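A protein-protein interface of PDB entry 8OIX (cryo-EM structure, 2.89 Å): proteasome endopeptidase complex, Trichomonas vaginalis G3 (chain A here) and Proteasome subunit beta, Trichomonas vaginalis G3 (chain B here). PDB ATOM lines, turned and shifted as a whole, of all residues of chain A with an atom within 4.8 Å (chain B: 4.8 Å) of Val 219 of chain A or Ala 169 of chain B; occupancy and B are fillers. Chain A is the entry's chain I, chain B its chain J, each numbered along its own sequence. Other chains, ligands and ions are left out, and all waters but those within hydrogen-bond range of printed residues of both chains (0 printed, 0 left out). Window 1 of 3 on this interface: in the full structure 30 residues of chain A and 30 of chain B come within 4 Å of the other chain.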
ATOM      1  N   ILE A 217      -4.322  -3.323  28.956  1.00  0.00           N
ATOM      2  CA  ILE A 217      -5.708  -2.939  28.714  1.00  0.00           C
ATOM      3  C   ILE A 217      -6.308  -3.922  27.721  1.00  0.00           C
ATOM      4  O   ILE A 217      -5.752  -4.139  26.638  1.00  0.00           O
ATOM      5  CB  ILE A 217      -5.813  -1.495  28.193  1.00  0.00           C
ATOM      6  CG1 ILE A 217      -5.666  -0.498  29.343  1.00  0.00           C
ATOM      7  CG2 ILE A 217      -7.134  -1.277  27.472  1.00  0.00           C
ATOM      8  CD1 ILE A 217      -5.694   0.946  28.902  1.00  0.00           C
ATOM      9  N   ASP A 218      -7.432  -4.526  28.092  1.00  0.00           N
ATOM     10  CA  ASP A 218      -8.126  -5.490  27.250  1.00  0.00           C
ATOM     11  C   ASP A 218      -9.414  -4.868  26.730  1.00  0.00           C
ATOM     12  O   ASP A 218     -10.197  -4.310  27.505  1.00  0.00           O
ATOM     13  CB  ASP A 218      -8.422  -6.776  28.024  1.00  0.00           C
ATOM     14  CG  ASP A 218      -7.166  -7.567  28.335  1.00  0.00           C
ATOM     15  OD1 ASP A 218      -6.217  -7.521  27.524  1.00  0.00           O
ATOM     16  OD2 ASP A 218      -7.124  -8.234  29.390  1.00  0.00           O
ATOM     17  N   VAL A 219      -9.625  -4.963  25.421  1.00  0.00           N
ATOM     18  CA  VAL A 219     -10.788  -4.366  24.774  1.00  0.00           C
ATOM     19  C   VAL A 219     -11.940  -5.358  24.801  1.00  0.00           C
ATOM     20  O   VAL A 219     -11.821  -6.478  24.292  1.00  0.00           O
ATOM     21  CB  VAL A 219     -10.468  -3.950  23.332  1.00  0.00           C
ATOM     22  CG1 VAL A 219     -11.680  -3.294  22.696  1.00  0.00           C
ATOM     23  CG2 VAL A 219      -9.286  -3.022  23.309  1.00  0.00           C
ATOM     24  N   GLU A 220     -13.055  -4.947  25.394  1.00  0.00           N
ATOM     25  CA  GLU A 220     -14.293  -5.711  25.355  1.00  0.00           C
ATOM     26  C   GLU A 220     -15.239  -5.010  24.388  1.00  0.00           C
ATOM     27  O   GLU A 220     -15.575  -3.838  24.584  1.00  0.00           O
ATOM     28  CB  GLU A 220     -14.905  -5.831  26.749  1.00  0.00           C
ATOM     29  CG  GLU A 220     -13.970  -6.488  27.758  1.00  0.00           C
ATOM     30  CD  GLU A 220     -14.603  -6.672  29.124  1.00  0.00           C
ATOM     31  OE1 GLU A 220     -15.843  -6.784  29.198  1.00  0.00           O
ATOM     32  OE2 GLU A 220     -13.858  -6.705  30.126  1.00  0.00           O
ATOM     33  N   VAL A 221     -15.651  -5.718  23.342  1.00  0.00           N
ATOM     34  CA  VAL A 221     -16.442  -5.130  22.268  1.00  0.00           C
ATOM     35  C   VAL A 221     -17.918  -5.379  22.558  1.00  0.00           C
ATOM     36  O   VAL A 221     -18.375  -6.525  22.569  1.00  0.00           O
ATOM     37  CB  VAL A 221     -16.042  -5.695  20.902  1.00  0.00           C
ATOM     38  CG1 VAL A 221     -16.943  -5.131  19.827  1.00  0.00           C
ATOM     39  CG2 VAL A 221     -14.587  -5.375  20.605  1.00  0.00           C
ATOM     40  N   PHE B 165      -7.405  -1.292  15.019  1.00  0.00           N
ATOM     41  CA  PHE B 165      -8.496  -1.296  15.985  1.00  0.00           C
ATOM     42  C   PHE B 165      -7.970  -1.514  17.393  1.00  0.00           C
ATOM     43  O   PHE B 165      -8.477  -0.920  18.349  1.00  0.00           O
ATOM     44  CB  PHE B 165      -9.518  -2.378  15.647  1.00  0.00           C
ATOM     45  CG  PHE B 165     -10.443  -2.698  16.785  1.00  0.00           C
ATOM     46  CD1 PHE B 165     -11.421  -1.800  17.170  1.00  0.00           C
ATOM     47  CD2 PHE B 165     -10.321  -3.887  17.481  1.00  0.00           C
ATOM     48  CE1 PHE B 165     -12.266  -2.084  18.222  1.00  0.00           C
ATOM     49  CE2 PHE B 165     -11.165  -4.177  18.534  1.00  0.00           C
ATOM     50  CZ  PHE B 165     -12.138  -3.273  18.904  1.00  0.00           C
ATOM     51  N   GLU B 166      -6.965  -2.376  17.540  1.00  0.00           N
ATOM     52  CA  GLU B 166      -6.446  -2.691  18.863  1.00  0.00           C
ATOM     53  C   GLU B 166      -5.949  -1.436  19.566  1.00  0.00           C
ATOM     54  O   GLU B 166      -6.379  -1.136  20.684  1.00  0.00           O
ATOM     55  CB  GLU B 166      -5.332  -3.734  18.756  1.00  0.00           C
ATOM     56  CG  GLU B 166      -5.179  -4.629  19.981  1.00  0.00           C
ATOM     57  CD  GLU B 166      -6.412  -5.470  20.281  1.00  0.00           C
ATOM     58  OE1 GLU B 166      -7.330  -5.537  19.436  1.00  0.00           O
ATOM     59  OE2 GLU B 166      -6.461  -6.072  21.374  1.00  0.00           O
ATOM     60  N   CYS B 167      -5.070  -0.665  18.918  1.00  0.00           N
ATOM     61  CA  CYS B 167      -4.637   0.560  19.595  1.00  0.00           C
ATOM     62  C   CYS B 167      -5.744   1.596  19.621  1.00  0.00           C
ATOM     63  O   CYS B 167      -5.918   2.266  20.631  1.00  0.00           O
ATOM     64  CB  CYS B 167      -3.379   1.186  19.002  1.00  0.00           C
ATOM     65  SG  CYS B 167      -3.009   2.909  19.697  1.00  0.00           S
ATOM     66  N   THR B 168      -6.501   1.772  18.541  1.00  0.00           N
ATOM     67  CA  THR B 168      -7.556   2.775  18.601  1.00  0.00           C
ATOM     68  C   THR B 168      -8.409   2.564  19.848  1.00  0.00           C
ATOM     69  O   THR B 168      -8.562   3.474  20.668  1.00  0.00           O
ATOM     70  CB  THR B 168      -8.400   2.727  17.331  1.00  0.00           C
ATOM     71  OG1 THR B 168      -7.555   2.405  16.222  1.00  0.00           O
ATOM     72  CG2 THR B 168      -9.028   4.080  17.075  1.00  0.00           C
ATOM     73  N   ALA B 169      -8.848   1.324  20.073  1.00  0.00           N
ATOM     74  CA  ALA B 169      -9.666   1.011  21.238  1.00  0.00           C
ATOM     75  C   ALA B 169      -8.886   1.149  22.544  1.00  0.00           C
ATOM     76  O   ALA B 169      -9.338   1.834  23.463  1.00  0.00           O
ATOM     77  CB  ALA B 169     -10.241  -0.396  21.099  1.00  0.00           C
ATOM     78  N   LYS B 170      -7.709   0.516  22.651  1.00  0.00           N
ATOM     79  CA  LYS B 170      -6.971   0.523  23.915  1.00  0.00           C
ATOM     80  C   LYS B 170      -6.497   1.924  24.270  1.00  0.00           C
ATOM     81  O   LYS B 170      -6.617   2.371  25.416  1.00  0.00           O
ATOM     82  CB  LYS B 170      -5.760  -0.408  23.824  1.00  0.00           C
ATOM     83  CG  LYS B 170      -6.060  -1.882  23.681  1.00  0.00           C
ATOM     84  CD  LYS B 170      -4.773  -2.688  23.639  1.00  0.00           C
ATOM     85  CE  LYS B 170      -5.050  -4.180  23.614  1.00  0.00           C
ATOM     86  NZ  LYS B 170      -3.980  -4.954  24.304  1.00  0.00           N
ATOM     87  N   CYS B 171      -5.919   2.610  23.291  1.00  0.00           N
ATOM     88  CA  CYS B 171      -5.405   3.957  23.447  1.00  0.00           C
ATOM     89  C   CYS B 171      -6.529   4.947  23.768  1.00  0.00           C
ATOM     90  O   CYS B 171      -6.378   5.800  24.656  1.00  0.00           O
ATOM     91  CB  CYS B 171      -4.630   4.300  22.159  1.00  0.00           C
ATOM     92  SG  CYS B 171      -3.341   2.977  21.728  1.00  0.00           S
ATOM     93  N   LEU B 172      -7.692   4.808  23.116  1.00  0.00           N
ATOM     94  CA  LEU B 172      -8.839   5.641  23.467  1.00  0.00           C
ATOM     95  C   LEU B 172      -9.357   5.324  24.864  1.00  0.00           C
ATOM     96  O   LEU B 172      -9.787   6.229  25.586  1.00  0.00           O
ATOM     97  CB  LEU B 172      -9.953   5.461  22.437  1.00  0.00           C
ATOM     98  CG  LEU B 172     -11.217   6.293  22.670  1.00  0.00           C
ATOM     99  CD1 LEU B 172     -11.124   7.628  21.950  1.00  0.00           C
ATOM    100  CD2 LEU B 172     -12.458   5.527  22.244  1.00  0.00           C
ATOM    101  N   ILE B 173      -9.359   4.047  25.250  1.00  0.00           N
ATOM    102  CA  ILE B 173      -9.786   3.669  26.594  1.00  0.00           C
ATOM    103  C   ILE B 173      -8.872   4.300  27.633  1.00  0.00           C
ATOM    104  O   ILE B 173      -9.334   4.852  28.638  1.00  0.00           O
ATOM    105  CB  ILE B 173      -9.830   2.134  26.729  1.00  0.00           C
ATOM    106  CG1 ILE B 173     -11.046   1.560  26.002  1.00  0.00           C
ATOM    107  CG2 ILE B 173      -9.829   1.718  28.182  1.00  0.00           C
ATOM    108  CD1 ILE B 173     -10.932   0.083  25.699  1.00  0.00           C
ATOM    109  N   VAL B 188     -15.606   2.627  17.677  1.00  0.00           N
ATOM    110  CA  VAL B 188     -14.443   2.657  16.799  1.00  0.00           C
ATOM    111  C   VAL B 188     -14.891   2.246  15.402  1.00  0.00           C
ATOM    112  O   VAL B 188     -15.380   1.128  15.205  1.00  0.00           O
ATOM    113  CB  VAL B 188     -13.325   1.733  17.306  1.00  0.00           C
ATOM    114  CG1 VAL B 188     -12.041   1.998  16.551  1.00  0.00           C
ATOM    115  CG2 VAL B 188     -13.122   1.903  18.803  1.00  0.00           C
ATOM    116  N   ILE B 201     -16.840  -0.463  21.687  1.00  0.00           N
ATOM    117  CA  ILE B 201     -15.935  -0.983  22.695  1.00  0.00           C
ATOM    118  C   ILE B 201     -16.413  -0.551  24.075  1.00  0.00           C
ATOM    119  O   ILE B 201     -17.085   0.475  24.247  1.00  0.00           O
ATOM    120  CB  ILE B 201     -14.488  -0.514  22.454  1.00  0.00           C
ATOM    121  CG1 ILE B 201     -14.399   1.002  22.621  1.00  0.00           C
ATOM    122  CG2 ILE B 201     -14.022  -0.927  21.074  1.00  0.00           C
ATOM    123  CD1 ILE B 201     -13.016   1.561  22.470  1.00  0.00           C
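O of Ile 217 of chain A lies within hydrogen-bond range of NZ of Lys 170 of chain B, 3.0 Å away.
The side-chain amino group (NZ) of Lys 170 of chain B is in salt-bridge range of the side-chain carboxylate (OE2) of Glu 166 of chain B. The side-chain sulfur (SG) of Cys 167 of chain B forms a disulfide with the side-chain sulfur (SG) of Cys 171 of chain B, at 2.1 Å.
Among the printed residues, pairs that only touch across the chains: Glu 220 of chain A with Ile 201 of chain B, Val 219 of chain A with Lys 170 of chain B, Val 219 of chain A with Ala 169 of chain B, Val 221 of chain A with Phe 165 of chain B, Val 219 of chain A with Ile 201 of chain B and Val 219 of chain A with Phe 165 of chain B.
Printed residues of chain B within 4 Å of Ile 217 of chain A: Lys 170. Of the printed residues of chain B, Val 219 of chain A touches Phe 165 (3.8 Å), Ala 169 (3.6 Å), Lys 170 (3.4 Å) and Ile 201 (3.7 Å). Printed residues of chain B within 4 Å of Glu 220 of chain A: Ile 201. Of the printed residues of chain A, Phe 165 of chain B touches Val 219 and Val 221. Ala 169 of chain B touches one residue of chain A. Printed residues of chain A within 4 Å of Lys 170 of chain B: Ile 217 and Val 219. Val 188 of chain B touches none of the printed residues of chain A. Of the printed residues of chain A, Ile 201 of chain B touches Val 219 (3.7 Å) and Glu 220 (3.4 Å). The nearest residue of chain B that does not touch Val 219 of chain A is Ile 173 of chain B (4.2 Å). The nearest printed residue of chain A that does not touch Ala 169 of chain B is Ile 217 of chain A (5.5 Å).
Hydrophobic or aromatic side chains of chain A that line the printed part of chain B: Ile 217, Val 219 and Val 221. Of the 11 printed residues of chain B, 4 touch a printed residue of chain A. Printed residues of chain B that touch a printed residue of chain A: Phe 165, Ala 169, Lys 170 and Ile 201. Hydrophobic or aromatic side chains of chain B within 4 Å of the printed part of chain A: Phe 165, Ala 169 and Ile 201. Among the printed residues, no Asp or Glu carboxylate lies within 4 Å of a Lys or Arg side-chain nitrogen of the other chain.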
